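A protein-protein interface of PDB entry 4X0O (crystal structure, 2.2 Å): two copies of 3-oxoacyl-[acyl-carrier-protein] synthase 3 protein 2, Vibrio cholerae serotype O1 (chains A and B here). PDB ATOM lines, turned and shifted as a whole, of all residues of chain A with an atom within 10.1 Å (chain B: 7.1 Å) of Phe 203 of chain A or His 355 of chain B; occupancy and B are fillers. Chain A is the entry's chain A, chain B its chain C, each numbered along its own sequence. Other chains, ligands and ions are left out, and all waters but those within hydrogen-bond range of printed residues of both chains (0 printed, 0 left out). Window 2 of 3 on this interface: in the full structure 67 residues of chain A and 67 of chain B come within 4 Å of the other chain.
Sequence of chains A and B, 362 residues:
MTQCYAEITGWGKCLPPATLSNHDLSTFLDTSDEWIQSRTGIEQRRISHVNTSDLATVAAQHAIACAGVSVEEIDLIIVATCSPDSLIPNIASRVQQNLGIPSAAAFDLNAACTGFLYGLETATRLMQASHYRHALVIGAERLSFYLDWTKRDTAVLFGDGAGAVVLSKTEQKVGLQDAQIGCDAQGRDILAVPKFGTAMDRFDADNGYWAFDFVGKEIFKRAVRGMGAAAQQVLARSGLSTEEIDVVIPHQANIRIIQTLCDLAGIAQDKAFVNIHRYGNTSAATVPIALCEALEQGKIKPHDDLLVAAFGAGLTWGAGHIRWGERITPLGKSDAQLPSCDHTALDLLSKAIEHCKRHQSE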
ATOM      1  N   GLY A 197     -28.769 -13.175  11.694  1.00  0.00           N
ATOM      2  CA  GLY A 197     -27.495 -12.491  11.801  1.00  0.00           C
ATOM      3  C   GLY A 197     -27.059 -12.548  13.255  1.00  0.00           C
ATOM      4  O   GLY A 197     -27.618 -13.325  14.036  1.00  0.00           O
ATOM      5  N   THR A 198     -26.075 -11.732  13.626  1.00  0.00           N
ATOM      6  CA  THR A 198     -25.487 -11.811  14.966  1.00  0.00           C
ATOM      7  C   THR A 198     -26.403 -11.210  16.050  1.00  0.00           C
ATOM      8  O   THR A 198     -26.100 -11.320  17.234  1.00  0.00           O
ATOM      9  CB  THR A 198     -24.090 -11.151  15.042  1.00  0.00           C
ATOM     10  OG1 THR A 198     -24.188  -9.753  14.750  1.00  0.00           O
ATOM     11  CG2 THR A 198     -23.141 -11.813  14.062  1.00  0.00           C
ATOM     12  N   ALA A 199     -27.503 -10.575  15.637  1.00  0.00           N
ATOM     13  CA  ALA A 199     -28.532 -10.123  16.567  1.00  0.00           C
ATOM     14  C   ALA A 199     -29.407 -11.269  17.082  1.00  0.00           C
ATOM     15  O   ALA A 199     -30.164 -11.080  18.037  1.00  0.00           O
ATOM     16  CB  ALA A 199     -29.411  -9.068  15.895  1.00  0.00           C
ATOM     17  N   MET A 200     -29.352 -12.426  16.424  1.00  0.00           N
ATOM     18  CA  MET A 200     -30.208 -13.552  16.782  1.00  0.00           C
ATOM     19  C   MET A 200     -29.661 -14.287  17.999  1.00  0.00           C
ATOM     20  O   MET A 200     -28.461 -14.236  18.263  1.00  0.00           O
ATOM     21  CB  MET A 200     -30.358 -14.528  15.607  1.00  0.00           C
ATOM     22  CG  MET A 200     -29.246 -15.549  15.450  1.00  0.00           C
ATOM     23  SD  MET A 200     -29.150 -16.189  13.774  1.00  0.00           S
ATOM     24  CE  MET A 200     -30.615 -17.221  13.697  1.00  0.00           C
ATOM     25  N   ASP A 201     -30.565 -14.911  18.753  1.00  0.00           N
ATOM     26  CA  ASP A 201     -30.184 -15.750  19.894  1.00  0.00           C
ATOM     27  C   ASP A 201     -29.705 -17.074  19.320  1.00  0.00           C
ATOM     28  O   ASP A 201     -30.487 -17.855  18.781  1.00  0.00           O
ATOM     29  CB  ASP A 201     -31.370 -15.946  20.839  1.00  0.00           C
ATOM     30  CG  ASP A 201     -30.968 -16.563  22.203  1.00  0.00           C
ATOM     31  OD1 ASP A 201     -29.881 -17.172  22.329  1.00  0.00           O
ATOM     32  OD2 ASP A 201     -31.760 -16.448  23.162  1.00  0.00           O
ATOM     33  N   ARG A 202     -28.402 -17.301  19.430  1.00  0.00           N
ATOM     34  CA  ARG A 202     -27.741 -18.444  18.818  1.00  0.00           C
ATOM     35  C   ARG A 202     -28.198 -19.803  19.369  1.00  0.00           C
ATOM     36  O   ARG A 202     -28.153 -20.808  18.655  1.00  0.00           O
ATOM     37  CB  ARG A 202     -26.223 -18.289  19.001  1.00  0.00           C
ATOM     38  CG  ARG A 202     -25.375 -19.462  18.553  1.00  0.00           C
ATOM     39  CD  ARG A 202     -23.910 -19.180  18.835  1.00  0.00           C
ATOM     40  NE  ARG A 202     -23.063 -20.360  18.657  1.00  0.00           N
ATOM     41  CZ  ARG A 202     -21.783 -20.419  18.999  1.00  0.00           C
ATOM     42  NH1 ARG A 202     -21.179 -19.360  19.536  1.00  0.00           N
ATOM     43  NH2 ARG A 202     -21.098 -21.547  18.829  1.00  0.00           N
ATOM     44  N   PHE A 203     -28.608 -19.832  20.629  1.00  0.00           N
ATOM     45  CA  PHE A 203     -28.936 -21.085  21.311  1.00  0.00           C
ATOM     46  C   PHE A 203     -30.421 -21.246  21.607  1.00  0.00           C
ATOM     47  O   PHE A 203     -30.808 -22.161  22.319  1.00  0.00           O
ATOM     48  CB  PHE A 203     -28.121 -21.185  22.601  1.00  0.00           C
ATOM     49  CG  PHE A 203     -26.639 -21.120  22.375  1.00  0.00           C
ATOM     50  CD1 PHE A 203     -25.967 -22.191  21.808  1.00  0.00           C
ATOM     51  CD2 PHE A 203     -25.918 -19.976  22.706  1.00  0.00           C
ATOM     52  CE1 PHE A 203     -24.603 -22.135  21.589  1.00  0.00           C
ATOM     53  CE2 PHE A 203     -24.549 -19.910  22.484  1.00  0.00           C
ATOM     54  CZ  PHE A 203     -23.891 -20.994  21.926  1.00  0.00           C
ATOM     55  N   ASP A 204     -31.249 -20.355  21.067  1.00  0.00           N
ATOM     56  CA  ASP A 204     -32.691 -20.510  21.157  1.00  0.00           C
ATOM     57  C   ASP A 204     -33.132 -21.474  20.054  1.00  0.00           C
ATOM     58  O   ASP A 204     -32.784 -21.293  18.880  1.00  0.00           O
ATOM     59  CB  ASP A 204     -33.379 -19.149  21.010  1.00  0.00           C
ATOM     60  CG  ASP A 204     -34.893 -19.227  21.158  1.00  0.00           C
ATOM     61  OD1 ASP A 204     -35.487 -20.315  20.977  1.00  0.00           O
ATOM     62  OD2 ASP A 204     -35.502 -18.180  21.462  1.00  0.00           O
ATOM     63  N   ALA A 205     -33.881 -22.506  20.437  1.00  0.00           N
ATOM     64  CA  ALA A 205     -34.343 -23.525  19.487  1.00  0.00           C
ATOM     65  C   ALA A 205     -35.396 -22.988  18.509  1.00  0.00           C
ATOM     66  O   ALA A 205     -35.596 -23.563  17.435  1.00  0.00           O
ATOM     67  CB  ALA A 205     -34.881 -24.740  20.233  1.00  0.00           C
ATOM     68  N   ASP A 206     -36.075 -21.904  18.891  1.00  0.00           N
ATOM     69  CA  ASP A 206     -37.037 -21.225  18.016  1.00  0.00           C
ATOM     70  C   ASP A 206     -36.420 -20.098  17.167  1.00  0.00           C
ATOM     71  O   ASP A 206     -37.154 -19.347  16.524  1.00  0.00           O
ATOM     72  CB  ASP A 206     -38.177 -20.634  18.851  1.00  0.00           C
ATOM     73  CG  ASP A 206     -39.008 -21.695  19.550  1.00  0.00           C
ATOM     74  OD1 ASP A 206     -38.992 -22.871  19.107  1.00  0.00           O
ATOM     75  OD2 ASP A 206     -39.690 -21.344  20.542  1.00  0.00           O
ATOM     76  N   ASN A 207     -35.094 -19.975  17.142  1.00  0.00           N
ATOM     77  CA  ASN A 207     -34.459 -18.842  16.448  1.00  0.00           C
ATOM     78  C   ASN A 207     -34.611 -18.870  14.924  1.00  0.00           C
ATOM     79  O   ASN A 207     -34.358 -17.871  14.260  1.00  0.00           O
ATOM     80  CB  ASN A 207     -32.978 -18.689  16.842  1.00  0.00           C
ATOM     81  CG  ASN A 207     -32.098 -19.814  16.332  1.00  0.00           C
ATOM     82  OD1 ASN A 207     -32.517 -20.652  15.536  1.00  0.00           O
ATOM     83  ND2 ASN A 207     -30.858 -19.839  16.804  1.00  0.00           N
ATOM     84  N   GLY A 208     -35.046 -20.007  14.387  1.00  0.00           N
ATOM     85  CA  GLY A 208     -35.364 -20.131  12.971  1.00  0.00           C
ATOM     86  C   GLY A 208     -36.690 -19.519  12.540  1.00  0.00           C
ATOM     87  O   GLY A 208     -36.912 -19.297  11.346  1.00  0.00           O
ATOM     88  N   PHE B 145     -19.936 -13.549  19.331  1.00  0.00           N
ATOM     89  CA  PHE B 145     -21.102 -14.309  18.837  1.00  0.00           C
ATOM     90  C   PHE B 145     -20.763 -15.710  18.318  1.00  0.00           C
ATOM     91  O   PHE B 145     -21.525 -16.662  18.535  1.00  0.00           O
ATOM     92  CB  PHE B 145     -21.824 -13.527  17.730  1.00  0.00           C
ATOM     93  CG  PHE B 145     -22.952 -14.291  17.082  1.00  0.00           C
ATOM     94  CD1 PHE B 145     -24.201 -14.348  17.674  1.00  0.00           C
ATOM     95  CD2 PHE B 145     -22.751 -14.992  15.910  1.00  0.00           C
ATOM     96  CE1 PHE B 145     -25.233 -15.072  17.089  1.00  0.00           C
ATOM     97  CE2 PHE B 145     -23.781 -15.708  15.317  1.00  0.00           C
ATOM     98  CZ  PHE B 145     -25.020 -15.751  15.907  1.00  0.00           C
ATOM     99  N   LEU B 147     -17.938 -17.792  18.835  1.00  0.00           N
ATOM    100  CA  LEU B 147     -16.931 -18.664  19.425  1.00  0.00           C
ATOM    101  C   LEU B 147     -17.484 -19.963  20.033  1.00  0.00           C
ATOM    102  O   LEU B 147     -18.617 -20.014  20.512  1.00  0.00           O
ATOM    103  CB  LEU B 147     -16.082 -17.900  20.442  1.00  0.00           C
ATOM    104  CG  LEU B 147     -15.334 -16.694  19.865  1.00  0.00           C
ATOM    105  CD1 LEU B 147     -14.500 -16.002  20.926  1.00  0.00           C
ATOM    106  CD2 LEU B 147     -14.457 -17.094  18.681  1.00  0.00           C
ATOM    107  N   TRP B 149     -17.000 -22.203  22.912  1.00  0.00           N
ATOM    108  CA  TRP B 149     -16.428 -22.005  24.232  1.00  0.00           C
ATOM    109  C   TRP B 149     -15.832 -23.284  24.831  1.00  0.00           C
ATOM    110  O   TRP B 149     -15.342 -23.250  25.951  1.00  0.00           O
ATOM    111  CB  TRP B 149     -17.463 -21.369  25.169  1.00  0.00           C
ATOM    112  CG  TRP B 149     -17.893 -20.034  24.686  1.00  0.00           C
ATOM    113  CD1 TRP B 149     -19.128 -19.687  24.219  1.00  0.00           C
ATOM    114  CD2 TRP B 149     -17.080 -18.873  24.568  1.00  0.00           C
ATOM    115  NE1 TRP B 149     -19.141 -18.377  23.842  1.00  0.00           N
ATOM    116  CE2 TRP B 149     -17.893 -17.851  24.038  1.00  0.00           C
ATOM    117  CE3 TRP B 149     -15.745 -18.586  24.870  1.00  0.00           C
ATOM    118  CZ2 TRP B 149     -17.414 -16.568  23.791  1.00  0.00           C
ATOM    119  CZ3 TRP B 149     -15.268 -17.308  24.628  1.00  0.00           C
ATOM    120  CH2 TRP B 149     -16.100 -16.315  24.090  1.00  0.00           C
ATOM    121  N   THR B 150     -15.876 -24.393  24.089  1.00  0.00           N
ATOM    122  CA  THR B 150     -15.157 -25.616  24.456  1.00  0.00           C
ATOM    123  C   THR B 150     -13.826 -25.761  23.715  1.00  0.00           C
ATOM    124  O   THR B 150     -13.060 -26.681  23.996  1.00  0.00           O
ATOM    125  CB  THR B 150     -16.004 -26.871  24.157  1.00  0.00           C
ATOM    126  OG1 THR B 150     -16.230 -26.998  22.744  1.00  0.00           O
ATOM    127  CG2 THR B 150     -17.356 -26.797  24.875  1.00  0.00           C
ATOM    128  N   ALA B 205     -32.340 -27.755  15.841  1.00  0.00           N
ATOM    129  CA  ALA B 205     -32.151 -27.164  17.172  1.00  0.00           C
ATOM    130  C   ALA B 205     -30.691 -27.133  17.620  1.00  0.00           C
ATOM    131  O   ALA B 205     -30.324 -26.343  18.490  1.00  0.00           O
ATOM    132  CB  ALA B 205     -33.011 -27.889  18.202  1.00  0.00           C
ATOM    133  N   ASN B 207     -28.267 -26.320  15.511  1.00  0.00           N
ATOM    134  CA  ASN B 207     -27.538 -25.566  14.469  1.00  0.00           C
ATOM    135  C   ASN B 207     -26.597 -24.496  15.026  1.00  0.00           C
ATOM    136  O   ASN B 207     -25.775 -23.960  14.299  1.00  0.00           O
ATOM    137  CB  ASN B 207     -28.500 -24.979  13.415  1.00  0.00           C
ATOM    138  CG  ASN B 207     -29.393 -23.874  13.959  1.00  0.00           C
ATOM    139  OD1 ASN B 207     -29.221 -23.399  15.083  1.00  0.00           O
ATOM    140  ND2 ASN B 207     -30.368 -23.472  13.161  1.00  0.00           N
ATOM    141  N   GLY B 208     -26.742 -24.186  16.314  1.00  0.00           N
ATOM    142  CA  GLY B 208     -25.857 -23.258  16.999  1.00  0.00           C
ATOM    143  C   GLY B 208     -24.496 -23.825  17.364  1.00  0.00           C
ATOM    144  O   GLY B 208     -23.572 -23.061  17.672  1.00  0.00           O
ATOM    145  N   TYR B 209     -24.359 -25.148  17.348  1.00  0.00           N
ATOM    146  CA  TYR B 209     -23.140 -25.791  17.804  1.00  0.00           C
ATOM    147  C   TYR B 209     -22.220 -26.080  16.629  1.00  0.00           C
ATOM    148  O   TYR B 209     -21.870 -27.227  16.363  1.00  0.00           O
ATOM    149  CB  TYR B 209     -23.494 -27.062  18.606  1.00  0.00           C
ATOM    150  CG  TYR B 209     -24.358 -26.718  19.808  1.00  0.00           C
ATOM    151  CD1 TYR B 209     -23.811 -26.084  20.912  1.00  0.00           C
ATOM    152  CD2 TYR B 209     -25.731 -26.965  19.805  1.00  0.00           C
ATOM    153  CE1 TYR B 209     -24.592 -25.739  22.005  1.00  0.00           C
ATOM    154  CE2 TYR B 209     -26.526 -26.620  20.889  1.00  0.00           C
ATOM    155  CZ  TYR B 209     -25.950 -26.005  21.983  1.00  0.00           C
ATOM    156  OH  TYR B 209     -26.717 -25.646  23.066  1.00  0.00           O
ATOM    157  N   TRP B 210     -21.801 -25.008  15.957  1.00  0.00           N
ATOM    158  CA  TRP B 210     -21.030 -25.095  14.712  1.00  0.00           C
ATOM    159  C   TRP B 210     -19.534 -25.193  14.962  1.00  0.00           C
ATOM    160  O   TRP B 210     -19.024 -24.743  15.995  1.00  0.00           O
ATOM    161  CB  TRP B 210     -21.331 -23.889  13.786  1.00  0.00           C
ATOM    162  CG  TRP B 210     -21.201 -22.517  14.440  1.00  0.00           C
ATOM    163  CD1 TRP B 210     -20.071 -21.962  14.959  1.00  0.00           C
ATOM    164  CD2 TRP B 210     -22.250 -21.563  14.656  1.00  0.00           C
ATOM    165  NE1 TRP B 210     -20.355 -20.708  15.493  1.00  0.00           N
ATOM    166  CE2 TRP B 210     -21.679 -20.440  15.297  1.00  0.00           C
ATOM    167  CE3 TRP B 210     -23.615 -21.546  14.359  1.00  0.00           C
ATOM    168  CZ2 TRP B 210     -22.419 -19.316  15.636  1.00  0.00           C
ATOM    169  CZ3 TRP B 210     -24.353 -20.418  14.691  1.00  0.00           C
ATOM    170  CH2 TRP B 210     -23.753 -19.319  15.321  1.00  0.00           C
ATOM    171  N   LEU B 349     -20.977 -13.934  28.788  1.00  0.00           N
ATOM    172  CA  LEU B 349     -20.786 -15.191  28.074  1.00  0.00           C
ATOM    173  C   LEU B 349     -21.412 -16.392  28.775  1.00  0.00           C
ATOM    174  O   LEU B 349     -21.498 -17.482  28.193  1.00  0.00           O
ATOM    175  CB  LEU B 349     -19.294 -15.434  27.872  1.00  0.00           C
ATOM    176  CG  LEU B 349     -18.535 -14.350  27.094  1.00  0.00           C
ATOM    177  CD1 LEU B 349     -17.081 -14.762  26.965  1.00  0.00           C
ATOM    178  CD2 LEU B 349     -19.152 -14.077  25.720  1.00  0.00           C
ATOM    179  N   SER B 350     -21.845 -16.182  30.017  1.00  0.00           N
ATOM    180  CA  SER B 350     -22.396 -17.240  30.868  1.00  0.00           C
ATOM    181  C   SER B 350     -23.278 -18.258  30.111  1.00  0.00           C
ATOM    182  O   SER B 350     -22.973 -19.453  30.089  1.00  0.00           O
ATOM    183  CB  SER B 350     -23.183 -16.604  32.024  1.00  0.00           C
ATOM    184  OG  SER B 350     -23.628 -17.588  32.934  1.00  0.00           O
ATOM    185  N   LYS B 351     -24.356 -17.774  29.506  1.00  0.00           N
ATOM    186  CA  LYS B 351     -25.305 -18.634  28.802  1.00  0.00           C
ATOM    187  C   LYS B 351     -24.638 -19.422  27.672  1.00  0.00           C
ATOM    188  O   LYS B 351     -24.777 -20.651  27.592  1.00  0.00           O
ATOM    189  CB  LYS B 351     -26.454 -17.796  28.234  1.00  0.00           C
ATOM    190  N   ALA B 352     -23.887 -18.714  26.825  1.00  0.00           N
ATOM    191  CA  ALA B 352     -23.185 -19.336  25.701  1.00  0.00           C
ATOM    192  C   ALA B 352     -22.207 -20.419  26.142  1.00  0.00           C
ATOM    193  O   ALA B 352     -22.174 -21.506  25.564  1.00  0.00           O
ATOM    194  CB  ALA B 352     -22.455 -18.274  24.881  1.00  0.00           C
ATOM    195  N   ILE B 353     -21.399 -20.109  27.153  1.00  0.00           N
ATOM    196  CA  ILE B 353     -20.459 -21.077  27.727  1.00  0.00           C
ATOM    197  C   ILE B 353     -21.192 -22.314  28.255  1.00  0.00           C
ATOM    198  O   ILE B 353     -20.814 -23.447  27.941  1.00  0.00           O
ATOM    199  CB  ILE B 353     -19.616 -20.447  28.852  1.00  0.00           C
ATOM    200  CG1 ILE B 353     -18.696 -19.360  28.279  1.00  0.00           C
ATOM    201  CG2 ILE B 353     -18.788 -21.512  29.571  1.00  0.00           C
ATOM    202  CD1 ILE B 353     -18.058 -18.472  29.333  1.00  0.00           C
ATOM    203  N   GLU B 354     -22.248 -22.095  29.036  1.00  0.00           N
ATOM    204  CA  GLU B 354     -23.065 -23.201  29.569  1.00  0.00           C
ATOM    205  C   GLU B 354     -23.628 -24.116  28.508  1.00  0.00           C
ATOM    206  O   GLU B 354     -23.631 -25.327  28.686  1.00  0.00           O
ATOM    207  CB  GLU B 354     -24.245 -22.673  30.352  1.00  0.00           C
ATOM    208  N   HIS B 355     -24.148 -23.523  27.433  1.00  0.00           N
ATOM    209  CA  HIS B 355     -24.707 -24.301  26.328  1.00  0.00           C
ATOM    210  C   HIS B 355     -23.635 -25.101  25.593  1.00  0.00           C
ATOM    211  O   HIS B 355     -23.850 -26.259  25.245  1.00  0.00           O
ATOM    212  CB  HIS B 355     -25.407 -23.391  25.335  1.00  0.00           C
ATOM    213  CG  HIS B 355     -26.798 -23.012  25.723  1.00  0.00           C
ATOM    214  ND1 HIS B 355     -27.110 -21.779  26.252  1.00  0.00           N
ATOM    215  CD2 HIS B 355     -27.972 -23.673  25.589  1.00  0.00           C
ATOM    216  CE1 HIS B 355     -28.414 -21.706  26.454  1.00  0.00           C
ATOM    217  NE2 HIS B 355     -28.961 -22.840  26.053  1.00  0.00           N
ATOM    218  N   CYS B 356     -22.486 -24.474  25.353  1.00  0.00           N
ATOM    219  CA  CYS B 356     -21.390 -25.136  24.667  1.00  0.00           C
ATOM    220  C   CYS B 356     -20.856 -26.320  25.483  1.00  0.00           C
ATOM    221  O   CYS B 356     -20.567 -27.380  24.923  1.00  0.00           O
ATOM    222  CB  CYS B 356     -20.266 -24.140  24.334  1.00  0.00           C
ATOM    223  SG  CYS B 356     -20.643 -23.006  22.964  1.00  0.00           S
ATOM    224  N   LYS B 357     -20.745 -26.145  26.797  1.00  0.00           N
ATOM    225  CA  LYS B 357     -20.275 -27.223  27.679  1.00  0.00           C
ATOM    226  C   LYS B 357     -21.309 -28.344  27.809  1.00  0.00           C
ATOM    227  O   LYS B 357     -20.956 -29.523  27.737  1.00  0.00           O
ATOM    228  CB  LYS B 357     -19.912 -26.676  29.055  1.00  0.00           C
ATOM    229  N   ARG B 358     -22.579 -27.976  27.996  1.00  0.00           N
ATOM    230  CA  ARG B 358     -23.669 -28.950  28.138  1.00  0.00           C
ATOM    231  C   ARG B 358     -23.865 -29.810  26.879  1.00  0.00           C
ATOM    232  O   ARG B 358     -24.194 -30.991  26.973  1.00  0.00           O
ATOM    233  CB  ARG B 358     -24.980 -28.240  28.497  1.00  0.00           C
ATOM    234  N   HIS B 359     -23.650 -29.219  25.708  1.00  0.00           N
ATOM    235  CA  HIS B 359     -23.803 -29.933  24.442  1.00  0.00           C
ATOM    236  C   HIS B 359     -22.658 -30.933  24.190  1.00  0.00           C
ATOM    237  O   HIS B 359     -22.868 -31.970  23.555  1.00  0.00           O
ATOM    238  CB  HIS B 359     -23.913 -28.929  23.272  1.00  0.00           C
ATOM    239  CG  HIS B 359     -24.027 -29.582  21.926  1.00  0.00           C
ATOM    240  ND1 HIS B 359     -25.222 -29.704  21.247  1.00  0.00           N
ATOM    241  CD2 HIS B 359     -23.093 -30.188  21.153  1.00  0.00           C
ATOM    242  CE1 HIS B 359     -25.017 -30.354  20.115  1.00  0.00           C
ATOM    243  NE2 HIS B 359     -23.736 -30.665  20.036  1.00  0.00           N
ATOM    244  N   GLN B 360     -21.458 -30.615  24.670  1.00  0.00           N
ATOM    245  CA  GLN B 360     -20.290 -31.485  24.488  1.00  0.00           C
ATOM    246  C   GLN B 360     -20.460 -32.827  25.217  1.00  0.00           C
ATOM    247  O   GLN B 360     -20.999 -32.878  26.321  1.00  0.00           O
ATOM    248  CB  GLN B 360     -19.036 -30.774  25.002  1.00  0.00           C
ATOM    249  CG  GLN B 360     -17.713 -31.455  24.662  1.00  0.00           C
ATOM    250  CD  GLN B 360     -16.512 -30.790  25.329  1.00  0.00           C
ATOM    251  OE1 GLN B 360     -16.656 -29.859  26.121  1.00  0.00           O
ATOM    252  NE2 GLN B 360     -15.318 -31.264  24.998  1.00  0.00           N
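The guanidinium group (NE) of Arg 202 of chain A lies within hydrogen-bond range of the backbone carbonyl oxygen (O) of Gly 208 of chain B. O of Phe 145 of chain B lies within hydrogen-bond range of NH1 of Arg 202 of chain A, at 2.9 Å. NH1 of Arg 202 of chain A is in hydrogen-bond range of O of Leu 147 of chain B, at 2.8 Å.
The backbone carbonyl oxygen (O) of Arg 202 of chain A sits at hydrogen-bond distance from the side-chain amide nitrogen (ND2) of Asn 207 of chain A (3.4 Å). SD of Met 200 of chain A sits at hydrogen-bond distance from N of Gly 197 of chain A. OD1 of Asp 201 of chain A sits close to N of Phe 203 of chain A, 3.4 Å away. A ring nitrogen (ND1) of His 355 of chain B lies within hydrogen-bond range of the backbone carbonyl oxygen of Lys 351 of chain B (2.9 Å). The backbone carbonyl oxygen of Ala 352 of chain B is in hydrogen-bond range of the side-chain sulfur of Cys 356 of chain B (3.4 Å). The side-chain sulfur (SG) of Cys 356 of chain B is in hydrogen-bond range of the backbone NH (N) of Trp 149 of chain B, at 3.7 Å.
CD1 of Phe 145 of chain B touches O of Thr 198 of chain A, at 3.6 Å. CE1 of Phe 145 of chain B touches O of Met 200 of chain A, at 3.5 Å. Arg 202 of chain A touches Trp 210 of chain B. Phe 203 of chain A touches Tyr 209 of chain B. Ala 352 of chain B touches Phe 203 of chain A (CA to CE2, 3.5 Å). CD1 of Phe 203 of chain A touches CB of His 355 of chain B, 3.8 Å away. Phe 203 of chain A touches Cys 356 of chain B (CZ to SG, 3.96 Å).
Phe 203 of chain A touches four residues of chain B. His 355 of chain B touches just one residue of chain A: Phe 203. No residue of chain A comes within 4 Å of Lys 351 of chain B. Ala 352 of chain B touches one residue of chain A. Glu 354 of chain B touches none of the printed residues of chain A. No residue of chain A comes within 4 Å of Arg 358 of chain B. Of the printed residues of chain A, Leu 147 of chain B touches Arg 202 (2.8 Å). Printed residues of chain B within 4 Å of Thr 198 of chain A: Phe 145. Of the printed residues of chain A, Tyr 209 of chain B touches Phe 203 (3.6 Å). Printed residues of chain A within 4 Å of Phe 145 of chain B: Thr 198, Met 200 and Arg 202. Asp 206 of chain A touches none of the printed residues of chain B. Asn 207 of chain A touches none of the printed residues of chain B. The nearest residue of chain B that does not touch Phe 203 of chain A is Gly 208 of chain B (4.2 Å). The nearest residue of chain A that does not touch His 355 of chain B is Asp 204 of chain A (6.0 Å). The nearest printed residue of chain A that does not touch Trp 210 of chain B is Met 200 of chain A (6.4 Å).
Of the 21 printed residues of chain B, 8 touch a printed residue of chain A. Printed residues of chain B that touch a printed residue of chain A: Phe 145, Leu 147, Gly 208, Tyr 209, Trp 210, Ala 352, His 355 and Cys 356. Hydrophobic or aromatic side chains of chain B that line the printed part of chain A: Phe 145, Tyr 209, Trp 210, Ala 352 and His 355. Of the 12 printed residues of chain A, 4 touch a printed residue of chain B. Among the printed residues, 10 pairs touch across the chains.
3 positions are printed for both chains.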
